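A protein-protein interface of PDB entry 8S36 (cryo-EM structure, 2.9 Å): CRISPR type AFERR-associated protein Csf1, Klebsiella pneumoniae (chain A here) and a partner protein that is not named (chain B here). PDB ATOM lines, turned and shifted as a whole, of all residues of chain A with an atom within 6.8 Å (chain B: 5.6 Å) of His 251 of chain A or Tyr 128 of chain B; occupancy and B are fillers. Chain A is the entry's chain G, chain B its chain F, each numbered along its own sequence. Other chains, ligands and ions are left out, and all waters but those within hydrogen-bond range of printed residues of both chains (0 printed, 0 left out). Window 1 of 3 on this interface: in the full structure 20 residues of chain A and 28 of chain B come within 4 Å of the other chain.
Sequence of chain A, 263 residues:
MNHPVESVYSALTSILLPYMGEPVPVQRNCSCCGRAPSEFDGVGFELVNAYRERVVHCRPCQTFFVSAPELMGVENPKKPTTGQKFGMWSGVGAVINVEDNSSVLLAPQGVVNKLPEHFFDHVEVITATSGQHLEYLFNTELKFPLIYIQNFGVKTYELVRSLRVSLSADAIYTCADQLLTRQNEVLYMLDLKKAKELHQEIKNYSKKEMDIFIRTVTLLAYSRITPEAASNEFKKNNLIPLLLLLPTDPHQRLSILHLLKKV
Hydrophobic or aromatic side chains of chain B within 4 Å of the printed part of chain A: Val 18, Ile 78, Ala 80, Pro 126, Tyr 128 and Val 224. Among the printed residues, 22 pairs touch across the chains. Among the printed residues, no Asp or Glu carboxylate lies within 4 Å of a Lys or Arg side-chain nitrogen of the other chain.
Among the printed residues, merely in contact across the chains: Gln 183 of chain A with Val 18 of chain B (3.9 Å), Gln 183 of chain A with Ile 19 of chain B (3.7 Å), Gln 183 of chain A with Pro 126 of chain B (3.6 Å), Val 186 of chain A with Pro 126 of chain B (3.4 Å), Val 186 of chain A with Tyr 128 of chain B (3.3 Å), Leu 187 of chain A with Pro 126 of chain B (3.6 Å), Ala 221 of chain A with Gly 79 of chain B (3.1 Å), Tyr 222 of chain A with Ala 80 of chain B (3.9 Å), Thr 248 of chain A with Val 224 of chain B (3.3 Å), Asp 249 of chain A with Val 224 of chain B (3.0 Å), Pro 250 of chain A with Ile 78 of chain B (3.7 Å), Pro 250 of chain A with Gly 79 of chain B (3.9 Å), Pro 250 of chain A with Tyr 128 of chain B (3.4 Å), Pro 250 of chain A with Val 224 of chain B (3.8 Å), His 251 of chain A with Ala 80 of chain B (3.5 Å), His 251 of chain A with Pro 126 of chain B (3.8 Å), His 251 of chain A with Ala 127 of chain B (3.8 Å), His 251 of chain A with Tyr 128 of chain B (3.7 Å) and Leu 254 of chain A with Ala 80 of chain B (3.4 Å).
His 251 of chain A touches just these residues of chain B: Ala 80 (3.5 Å), Thr 81 (3.2 Å), Pro 126 (3.8 Å), Ala 127 (3.8 Å) and Tyr 128 (3.7 Å). Of the printed residues of chain B, Thr 248 of chain A touches Val 224 (3.3 Å). Printed residues of chain B within 4 Å of Ala 221 of chain A: Gly 79 and Ala 80. Printed residues of chain A within 4 Å of Ile 78 of chain B: Pro 250. Val 17 of chain B touches none of the printed residues of chain A. The nearest residue of chain B that does not touch His 251 of chain A is Thr 82 of chain B (4.6 Å). The nearest printed residue of chain B that does not touch Leu 254 of chain A is Thr 81 of chain B (6.6 Å).
OH of Tyr 128 of chain B sits close to OD1 of Asp 249 of chain A. N of Ala 80 of chain B is in hydrogen-bond range of O of Ala 221 of chain A (2.4 Å). O of Thr 81 of chain B sits at hydrogen-bond distance from NE2 of His 251 of chain A (3.2 Å).
The backbone carbonyl oxygen (O) of His 251 of chain A is in hydrogen-bond range of the side-chain hydroxyl (OG) of Ser 255 of chain A (2.9 Å). The backbone NH of Ser 129 of chain B sits at hydrogen-bond distance from the backbone carbonyl oxygen of Gly 79 of chain B (3.0 Å). The side-chain hydroxyl (OG) of Ser 129 of chain B sits at hydrogen-bond distance from the side-chain hydroxyl (OG1) of Thr 81 of chain B (2.9 Å). The side-chain carboxylate of Asp 249 of chain A sits at hydrogen-bond distance from the backbone NH of His 251 of chain A, 2.7 Å away. The backbone carbonyl oxygen (O) of Val 186 of chain A lies close to the side-chain amide oxygen (OE1) of Gln 252 of chain A (3.1 Å). N of Tyr 128 of chain B is in hydrogen-bond range of O of Val 17 of chain B (2.8 Å).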
ATOM      1  N   GLN A 183     -17.428  12.392 -11.667  1.00  0.00           N
ATOM      2  CA  GLN A 183     -16.857  13.228 -12.708  1.00  0.00           C
ATOM      3  C   GLN A 183     -17.012  12.647 -14.102  1.00  0.00           C
ATOM      4  O   GLN A 183     -16.898  13.391 -15.084  1.00  0.00           O
ATOM      5  CB  GLN A 183     -15.374  13.451 -12.430  1.00  0.00           C
ATOM      6  CG  GLN A 183     -15.114  14.251 -11.182  1.00  0.00           C
ATOM      7  CD  GLN A 183     -15.268  13.453  -9.905  1.00  0.00           C
ATOM      8  OE1 GLN A 183     -16.134  13.740  -9.080  1.00  0.00           O
ATOM      9  NE2 GLN A 183     -14.417  12.450  -9.729  1.00  0.00           N
ATOM     10  N   VAL A 186     -21.311  11.394 -16.578  1.00  0.00           N
ATOM     11  CA  VAL A 186     -21.978  12.005 -17.724  1.00  0.00           C
ATOM     12  C   VAL A 186     -21.721  11.188 -18.983  1.00  0.00           C
ATOM     13  O   VAL A 186     -22.590  11.074 -19.855  1.00  0.00           O
ATOM     14  CB  VAL A 186     -21.529  13.468 -17.893  1.00  0.00           C
ATOM     15  CG1 VAL A 186     -20.039  13.553 -18.210  1.00  0.00           C
ATOM     16  CG2 VAL A 186     -22.348  14.148 -18.978  1.00  0.00           C
ATOM     17  N   LEU A 187     -20.526  10.605 -19.099  1.00  0.00           N
ATOM     18  CA  LEU A 187     -20.250   9.697 -20.205  1.00  0.00           C
ATOM     19  C   LEU A 187     -21.003   8.385 -20.059  1.00  0.00           C
ATOM     20  O   LEU A 187     -21.225   7.697 -21.060  1.00  0.00           O
ATOM     21  CB  LEU A 187     -18.750   9.416 -20.311  1.00  0.00           C
ATOM     22  CG  LEU A 187     -17.980  10.147 -21.416  1.00  0.00           C
ATOM     23  CD1 LEU A 187     -16.491   9.856 -21.302  1.00  0.00           C
ATOM     24  CD2 LEU A 187     -18.489   9.758 -22.797  1.00  0.00           C
ATOM     25  N   MET A 189     -24.110   8.103 -18.508  1.00  0.00           N
ATOM     26  CA  MET A 189     -25.530   8.367 -18.315  1.00  0.00           C
ATOM     27  C   MET A 189     -26.194   8.371 -19.682  1.00  0.00           C
ATOM     28  O   MET A 189     -25.848   9.189 -20.541  1.00  0.00           O
ATOM     29  CB  MET A 189     -25.767   9.704 -17.613  1.00  0.00           C
ATOM     30  CG  MET A 189     -27.016   9.735 -16.744  1.00  0.00           C
ATOM     31  SD  MET A 189     -26.820   8.935 -15.137  1.00  0.00           S
ATOM     32  CE  MET A 189     -25.483   9.883 -14.413  1.00  0.00           C
ATOM     33  N   ALA A 221     -19.801  20.051 -30.679  1.00  0.00           N
ATOM     34  CA  ALA A 221     -19.437  19.432 -29.411  1.00  0.00           C
ATOM     35  C   ALA A 221     -17.936  19.200 -29.314  1.00  0.00           C
ATOM     36  O   ALA A 221     -17.376  19.229 -28.214  1.00  0.00           O
ATOM     37  CB  ALA A 221     -20.188  18.113 -29.236  1.00  0.00           C
ATOM     38  N   TYR A 222     -17.271  18.957 -30.440  1.00  0.00           N
ATOM     39  CA  TYR A 222     -15.818  18.867 -30.479  1.00  0.00           C
ATOM     40  C   TYR A 222     -15.159  20.211 -30.771  1.00  0.00           C
ATOM     41  O   TYR A 222     -13.938  20.262 -30.952  1.00  0.00           O
ATOM     42  CB  TYR A 222     -15.383  17.836 -31.525  1.00  0.00           C
ATOM     43  CG  TYR A 222     -15.745  16.409 -31.175  1.00  0.00           C
ATOM     44  CD1 TYR A 222     -15.406  15.865 -29.943  1.00  0.00           C
ATOM     45  CD2 TYR A 222     -16.425  15.606 -32.079  1.00  0.00           C
ATOM     46  CE1 TYR A 222     -15.737  14.564 -29.621  1.00  0.00           C
ATOM     47  CE2 TYR A 222     -16.759  14.303 -31.766  1.00  0.00           C
ATOM     48  CZ  TYR A 222     -16.412  13.787 -30.536  1.00  0.00           C
ATOM     49  OH  TYR A 222     -16.742  12.490 -30.219  1.00  0.00           O
ATOM     50  N   THR A 248     -27.912  20.619 -22.868  1.00  0.00           N
ATOM     51  CA  THR A 248     -26.863  21.620 -22.999  1.00  0.00           C
ATOM     52  C   THR A 248     -25.477  21.017 -22.822  1.00  0.00           C
ATOM     53  O   THR A 248     -24.498  21.590 -23.314  1.00  0.00           O
ATOM     54  CB  THR A 248     -27.076  22.737 -21.979  1.00  0.00           C
ATOM     55  OG1 THR A 248     -28.449  23.148 -21.994  1.00  0.00           O
ATOM     56  CG2 THR A 248     -26.189  23.928 -22.296  1.00  0.00           C
ATOM     57  N   ASP A 249     -25.373  19.884 -22.146  1.00  0.00           N
ATOM     58  CA  ASP A 249     -24.086  19.231 -21.949  1.00  0.00           C
ATOM     59  C   ASP A 249     -23.579  18.678 -23.277  1.00  0.00           C
ATOM     60  O   ASP A 249     -24.274  17.862 -23.895  1.00  0.00           O
ATOM     61  CB  ASP A 249     -24.238  18.115 -20.922  1.00  0.00           C
ATOM     62  CG  ASP A 249     -22.915  17.509 -20.513  1.00  0.00           C
ATOM     63  OD1 ASP A 249     -22.197  16.987 -21.391  1.00  0.00           O
ATOM     64  OD2 ASP A 249     -22.599  17.548 -19.307  1.00  0.00           O
ATOM     65  N   PRO A 250     -22.388  19.062 -23.748  1.00  0.00           N
ATOM     66  CA  PRO A 250     -21.911  18.511 -25.026  1.00  0.00           C
ATOM     67  C   PRO A 250     -21.658  17.016 -24.986  1.00  0.00           C
ATOM     68  O   PRO A 250     -21.840  16.340 -26.004  1.00  0.00           O
ATOM     69  CB  PRO A 250     -20.622  19.301 -25.289  1.00  0.00           C
ATOM     70  CG  PRO A 250     -20.161  19.710 -23.956  1.00  0.00           C
ATOM     71  CD  PRO A 250     -21.406  19.996 -23.170  1.00  0.00           C
ATOM     72  N   HIS A 251     -21.226  16.475 -23.846  1.00  0.00           N
ATOM     73  CA  HIS A 251     -20.996  15.036 -23.770  1.00  0.00           C
ATOM     74  C   HIS A 251     -22.310  14.268 -23.842  1.00  0.00           C
ATOM     75  O   HIS A 251     -22.385  13.214 -24.484  1.00  0.00           O
ATOM     76  CB  HIS A 251     -20.230  14.690 -22.493  1.00  0.00           C
ATOM     77  CG  HIS A 251     -18.744  14.694 -22.669  1.00  0.00           C
ATOM     78  ND1 HIS A 251     -18.065  13.660 -23.276  1.00  0.00           N
ATOM     79  CD2 HIS A 251     -17.808  15.608 -22.324  1.00  0.00           C
ATOM     80  CE1 HIS A 251     -16.774  13.936 -23.295  1.00  0.00           C
ATOM     81  NE2 HIS A 251     -16.591  15.112 -22.723  1.00  0.00           N
ATOM     82  N   GLN A 252     -23.358  14.783 -23.201  1.00  0.00           N
ATOM     83  CA  GLN A 252     -24.677  14.181 -23.360  1.00  0.00           C
ATOM     84  C   GLN A 252     -25.139  14.279 -24.807  1.00  0.00           C
ATOM     85  O   GLN A 252     -25.754  13.344 -25.338  1.00  0.00           O
ATOM     86  CB  GLN A 252     -25.684  14.860 -22.433  1.00  0.00           C
ATOM     87  CG  GLN A 252     -25.395  14.670 -20.954  1.00  0.00           C
ATOM     88  CD  GLN A 252     -26.038  13.420 -20.391  1.00  0.00           C
ATOM     89  OE1 GLN A 252     -25.352  12.480 -19.993  1.00  0.00           O
ATOM     90  NE2 GLN A 252     -27.365  13.404 -20.351  1.00  0.00           N
ATOM     91  N   ARG A 253     -24.854  15.408 -25.460  1.00  0.00           N
ATOM     92  CA  ARG A 253     -25.184  15.549 -26.874  1.00  0.00           C
ATOM     93  C   ARG A 253     -24.492  14.471 -27.695  1.00  0.00           C
ATOM     94  O   ARG A 253     -25.109  13.844 -28.562  1.00  0.00           O
ATOM     95  CB  ARG A 253     -24.779  16.936 -27.375  1.00  0.00           C
ATOM     96  CG  ARG A 253     -25.638  18.075 -26.865  1.00  0.00           C
ATOM     97  CD  ARG A 253     -25.166  19.399 -27.438  1.00  0.00           C
ATOM     98  NE  ARG A 253     -26.118  20.477 -27.199  1.00  0.00           N
ATOM     99  CZ  ARG A 253     -26.155  21.615 -27.880  1.00  0.00           C
ATOM    100  NH1 ARG A 253     -25.298  21.866 -28.857  1.00  0.00           N
ATOM    101  NH2 ARG A 253     -27.074  22.525 -27.573  1.00  0.00           N
ATOM    102  N   LEU A 254     -23.206  14.237 -27.428  1.00  0.00           N
ATOM    103  CA  LEU A 254     -22.470  13.217 -28.168  1.00  0.00           C
ATOM    104  C   LEU A 254     -23.028  11.828 -27.891  1.00  0.00           C
ATOM    105  O   LEU A 254     -23.122  10.998 -28.800  1.00  0.00           O
ATOM    106  CB  LEU A 254     -20.986  13.276 -27.808  1.00  0.00           C
ATOM    107  CG  LEU A 254     -20.210  14.484 -28.335  1.00  0.00           C
ATOM    108  CD1 LEU A 254     -18.842  14.559 -27.682  1.00  0.00           C
ATOM    109  CD2 LEU A 254     -20.075  14.425 -29.848  1.00  0.00           C
ATOM    110  N   SER A 255     -23.407  11.558 -26.641  1.00  0.00           N
ATOM    111  CA  SER A 255     -23.967  10.252 -26.306  1.00  0.00           C
ATOM    112  C   SER A 255     -25.269  10.009 -27.060  1.00  0.00           C
ATOM    113  O   SER A 255     -25.463   8.952 -27.677  1.00  0.00           O
ATOM    114  CB  SER A 255     -24.190  10.152 -24.798  1.00  0.00           C
ATOM    115  OG  SER A 255     -22.981  10.368 -24.090  1.00  0.00           O
ATOM    116  N   ILE A 256     -26.163  10.998 -27.059  1.00  0.00           N
ATOM    117  CA  ILE A 256     -27.449  10.786 -27.713  1.00  0.00           C
ATOM    118  C   ILE A 256     -27.276  10.778 -29.225  1.00  0.00           C
ATOM    119  O   ILE A 256     -28.031  10.108 -29.936  1.00  0.00           O
ATOM    120  CB  ILE A 256     -28.491  11.825 -27.255  1.00  0.00           C
ATOM    121  CG1 ILE A 256     -28.106  13.250 -27.660  1.00  0.00           C
ATOM    122  CG2 ILE A 256     -28.683  11.745 -25.746  1.00  0.00           C
ATOM    123  CD1 ILE A 256     -29.269  14.204 -27.615  1.00  0.00           C
ATOM    124  N   LEU A 257     -26.302  11.522 -29.750  1.00  0.00           N
ATOM    125  CA  LEU A 257     -26.036  11.456 -31.180  1.00  0.00           C
ATOM    126  C   LEU A 257     -25.495  10.090 -31.579  1.00  0.00           C
ATOM    127  O   LEU A 257     -25.845   9.570 -32.641  1.00  0.00           O
ATOM    128  CB  LEU A 257     -25.057  12.555 -31.589  1.00  0.00           C
ATOM    129  CG  LEU A 257     -25.697  13.751 -32.293  1.00  0.00           C
ATOM    130  CD1 LEU A 257     -26.426  14.633 -31.295  1.00  0.00           C
ATOM    131  CD2 LEU A 257     -24.646  14.540 -33.049  1.00  0.00           C
ATOM    132  N   SER B  13     -11.503  31.007 -19.864  1.00  0.00           N
ATOM    133  CA  SER B  13     -11.174  29.618 -19.572  1.00  0.00           C
ATOM    134  C   SER B  13      -9.901  29.230 -20.309  1.00  0.00           C
ATOM    135  O   SER B  13      -9.841  29.300 -21.541  1.00  0.00           O
ATOM    136  CB  SER B  13     -12.312  28.698 -19.994  1.00  0.00           C
ATOM    137  OG  SER B  13     -12.367  27.550 -19.166  1.00  0.00           O
ATOM    138  N   THR B  15      -8.201  26.105 -19.409  1.00  0.00           N
ATOM    139  CA  THR B  15      -8.148  24.652 -19.402  1.00  0.00           C
ATOM    140  C   THR B  15      -9.557  24.078 -19.445  1.00  0.00           C
ATOM    141  O   THR B  15     -10.504  24.728 -18.994  1.00  0.00           O
ATOM    142  CB  THR B  15      -7.426  24.148 -18.143  1.00  0.00           C
ATOM    143  OG1 THR B  15      -6.236  24.917 -17.933  1.00  0.00           O
ATOM    144  CG2 THR B  15      -7.062  22.677 -18.252  1.00  0.00           C
ATOM    145  N   PRO B  16      -9.731  22.867 -19.981  1.00  0.00           N
ATOM    146  CA  PRO B  16     -11.041  22.213 -19.885  1.00  0.00           C
ATOM    147  C   PRO B  16     -11.455  21.984 -18.439  1.00  0.00           C
ATOM    148  O   PRO B  16     -10.625  21.748 -17.560  1.00  0.00           O
ATOM    149  CB  PRO B  16     -10.835  20.885 -20.629  1.00  0.00           C
ATOM    150  CG  PRO B  16      -9.386  20.809 -20.965  1.00  0.00           C
ATOM    151  CD  PRO B  16      -8.884  22.199 -20.982  1.00  0.00           C
ATOM    152  N   VAL B  17     -12.764  22.060 -18.205  1.00  0.00           N
ATOM    153  CA  VAL B  17     -13.346  22.065 -16.865  1.00  0.00           C
ATOM    154  C   VAL B  17     -14.010  20.715 -16.629  1.00  0.00           C
ATOM    155  O   VAL B  17     -15.010  20.384 -17.277  1.00  0.00           O
ATOM    156  CB  VAL B  17     -14.358  23.207 -16.696  1.00  0.00           C
ATOM    157  CG1 VAL B  17     -14.898  23.233 -15.276  1.00  0.00           C
ATOM    158  CG2 VAL B  17     -13.734  24.547 -17.058  1.00  0.00           C
ATOM    159  N   VAL B  18     -13.463  19.935 -15.699  1.00  0.00           N
ATOM    160  CA  VAL B  18     -14.059  18.659 -15.307  1.00  0.00           C
ATOM    161  C   VAL B  18     -15.150  18.935 -14.277  1.00  0.00           C
ATOM    162  O   VAL B  18     -14.861  19.354 -13.154  1.00  0.00           O
ATOM    163  CB  VAL B  18     -13.004  17.696 -14.749  1.00  0.00           C
ATOM    164  CG1 VAL B  18     -13.644  16.370 -14.370  1.00  0.00           C
ATOM    165  CG2 VAL B  18     -11.887  17.485 -15.757  1.00  0.00           C
ATOM    166  N   ILE B  19     -16.402  18.685 -14.649  1.00  0.00           N
ATOM    167  CA  ILE B  19     -17.542  18.913 -13.765  1.00  0.00           C
ATOM    168  C   ILE B  19     -17.824  17.632 -12.989  1.00  0.00           C
ATOM    169  O   ILE B  19     -18.053  16.574 -13.584  1.00  0.00           O
ATOM    170  CB  ILE B  19     -18.782  19.358 -14.554  1.00  0.00           C
ATOM    171  CG1 ILE B  19     -18.469  20.585 -15.414  1.00  0.00           C
ATOM    172  CG2 ILE B  19     -19.935  19.653 -13.607  1.00  0.00           C
ATOM    173  CD1 ILE B  19     -18.282  21.861 -14.648  1.00  0.00           C
ATOM    174  N   PHE B  70     -21.319  28.341 -18.370  1.00  0.00           N
ATOM    175  CA  PHE B  70     -20.313  28.577 -19.390  1.00  0.00           C
ATOM    176  C   PHE B  70     -20.747  29.722 -20.296  1.00  0.00           C
ATOM    177  O   PHE B  70     -21.854  29.715 -20.840  1.00  0.00           O
ATOM    178  CB  PHE B  70     -20.081  27.310 -20.209  1.00  0.00           C
ATOM    179  CG  PHE B  70     -19.549  26.162 -19.404  1.00  0.00           C
ATOM    180  CD1 PHE B  70     -18.198  26.065 -19.120  1.00  0.00           C
ATOM    181  CD2 PHE B  70     -20.399  25.178 -18.933  1.00  0.00           C
ATOM    182  CE1 PHE B  70     -17.707  25.009 -18.381  1.00  0.00           C
ATOM    183  CE2 PHE B  70     -19.912  24.120 -18.193  1.00  0.00           C
ATOM    184  CZ  PHE B  70     -18.564  24.034 -17.918  1.00  0.00           C
ATOM    185  N   ILE B  78     -19.237  25.612 -26.130  1.00  0.00           N
ATOM    186  CA  ILE B  78     -18.977  24.522 -25.199  1.00  0.00           C
ATOM    187  C   ILE B  78     -18.520  23.299 -25.981  1.00  0.00           C
ATOM    188  O   ILE B  78     -19.157  22.896 -26.964  1.00  0.00           O
ATOM    189  CB  ILE B  78     -20.229  24.226 -24.359  1.00  0.00           C
ATOM    190  CG1 ILE B  78     -19.882  23.338 -23.161  1.00  0.00           C
ATOM    191  CG2 ILE B  78     -21.307  23.559 -25.201  1.00  0.00           C
ATOM    192  CD1 ILE B  78     -19.299  24.090 -21.991  1.00  0.00           C
ATOM    193  N   GLY B  79     -17.403  22.717 -25.563  1.00  0.00           N
ATOM    194  CA  GLY B  79     -16.832  21.580 -26.257  1.00  0.00           C
ATOM    195  C   GLY B  79     -16.586  20.419 -25.318  1.00  0.00           C
ATOM    196  O   GLY B  79     -16.371  20.593 -24.120  1.00  0.00           O
ATOM    197  N   ALA B  80     -16.615  19.220 -25.890  1.00  0.00           N
ATOM    198  CA  ALA B  80     -16.444  17.970 -25.152  1.00  0.00           C
ATOM    199  C   ALA B  80     -14.989  17.532 -25.274  1.00  0.00           C
ATOM    200  O   ALA B  80     -14.581  16.980 -26.299  1.00  0.00           O
ATOM    201  CB  ALA B  80     -17.391  16.896 -25.676  1.00  0.00           C
ATOM    202  N   THR B  81     -14.209  17.777 -24.229  1.00  0.00           N
ATOM    203  CA  THR B  81     -12.811  17.385 -24.157  1.00  0.00           C
ATOM    204  C   THR B  81     -12.660  16.349 -23.051  1.00  0.00           C
ATOM    205  O   THR B  81     -13.572  16.125 -22.256  1.00  0.00           O
ATOM    206  CB  THR B  81     -11.915  18.602 -23.894  1.00  0.00           C
ATOM    207  OG1 THR B  81     -12.346  19.698 -24.710  1.00  0.00           O
ATOM    208  CG2 THR B  81     -10.458  18.289 -24.212  1.00  0.00           C
ATOM    209  N   THR B  82     -11.522  15.663 -23.041  1.00  0.00           N
ATOM    210  CA  THR B  82     -11.234  14.659 -22.025  1.00  0.00           C
ATOM    211  C   THR B  82      -9.996  15.078 -21.249  1.00  0.00           C
ATOM    212  O   THR B  82      -8.904  15.182 -21.819  1.00  0.00           O
ATOM    213  CB  THR B  82     -11.039  13.278 -22.648  1.00  0.00           C
ATOM    214  OG1 THR B  82     -10.103  13.365 -23.725  1.00  0.00           O
ATOM    215  CG2 THR B  82     -12.360  12.735 -23.169  1.00  0.00           C
ATOM    216  N   PRO B 126     -14.591  13.277 -18.504  1.00  0.00           N
ATOM    217  CA  PRO B 126     -15.272  14.330 -19.265  1.00  0.00           C
ATOM    218  C   PRO B 126     -14.939  15.717 -18.739  1.00  0.00           C
ATOM    219  O   PRO B 126     -14.983  15.974 -17.534  1.00  0.00           O
ATOM    220  CB  PRO B 126     -16.753  13.996 -19.075  1.00  0.00           C
ATOM    221  CG  PRO B 126     -16.777  12.538 -18.874  1.00  0.00           C
ATOM    222  CD  PRO B 126     -15.504  12.172 -18.171  1.00  0.00           C
ATOM    223  N   ALA B 127     -14.602  16.615 -19.658  1.00  0.00           N
ATOM    224  CA  ALA B 127     -14.335  18.010 -19.364  1.00  0.00           C
ATOM    225  C   ALA B 127     -15.032  18.861 -20.413  1.00  0.00           C
ATOM    226  O   ALA B 127     -15.201  18.437 -21.561  1.00  0.00           O
ATOM    227  CB  ALA B 127     -12.836  18.301 -19.341  1.00  0.00           C
ATOM    228  N   TYR B 128     -15.438  20.059 -20.013  1.00  0.00           N
ATOM    229  CA  TYR B 128     -16.126  20.985 -20.901  1.00  0.00           C
ATOM    230  C   TYR B 128     -15.247  22.207 -21.112  1.00  0.00           C
ATOM    231  O   TYR B 128     -14.857  22.873 -20.148  1.00  0.00           O
ATOM    232  CB  TYR B 128     -17.485  21.370 -20.326  1.00  0.00           C
ATOM    233  CG  TYR B 128     -18.270  20.160 -19.902  1.00  0.00           C
ATOM    234  CD1 TYR B 128     -18.885  19.349 -20.837  1.00  0.00           C
ATOM    235  CD2 TYR B 128     -18.375  19.816 -18.569  1.00  0.00           C
ATOM    236  CE1 TYR B 128     -19.596  18.235 -20.455  1.00  0.00           C
ATOM    237  CE2 TYR B 128     -19.084  18.706 -18.173  1.00  0.00           C
ATOM    238  CZ  TYR B 128     -19.691  17.917 -19.120  1.00  0.00           C
ATOM    239  OH  TYR B 128     -20.403  16.807 -18.729  1.00  0.00           O
ATOM    240  N   SER B 129     -14.938  22.491 -22.373  1.00  0.00           N
ATOM    241  CA  SER B 129     -13.991  23.530 -22.761  1.00  0.00           C
ATOM    242  C   SER B 129     -14.767  24.632 -23.474  1.00  0.00           C
ATOM    243  O   SER B 129     -14.923  24.614 -24.695  1.00  0.00           O
ATOM    244  CB  SER B 129     -12.893  22.958 -23.650  1.00  0.00           C
ATOM    245  OG  SER B 129     -13.435  22.409 -24.838  1.00  0.00           O
ATOM    246  N   ALA B 130     -15.255  25.593 -22.696  1.00  0.00           N
ATOM    247  CA  ALA B 130     -15.928  26.768 -23.213  1.00  0.00           C
ATOM    248  C   ALA B 130     -15.042  27.992 -23.027  1.00  0.00           C
ATOM    249  O   ALA B 130     -14.234  28.038 -22.096  1.00  0.00           O
ATOM    250  CB  ALA B 130     -17.267  27.003 -22.507  1.00  0.00           C
ATOM    251  N   VAL B 224     -24.060  21.427 -16.938  1.00  0.00           N
ATOM    252  CA  VAL B 224     -23.516  22.230 -18.027  1.00  0.00           C
ATOM    253  C   VAL B 224     -24.599  23.208 -18.456  1.00  0.00           C
ATOM    254  O   VAL B 224     -25.609  22.809 -19.047  1.00  0.00           O
ATOM    255  CB  VAL B 224     -23.059  21.361 -19.205  1.00  0.00           C
ATOM    256  CG1 VAL B 224     -22.618  22.237 -20.368  1.00  0.00           C
ATOM    257  CG2 VAL B 224     -21.940  20.432 -18.776  1.00  0.00           C
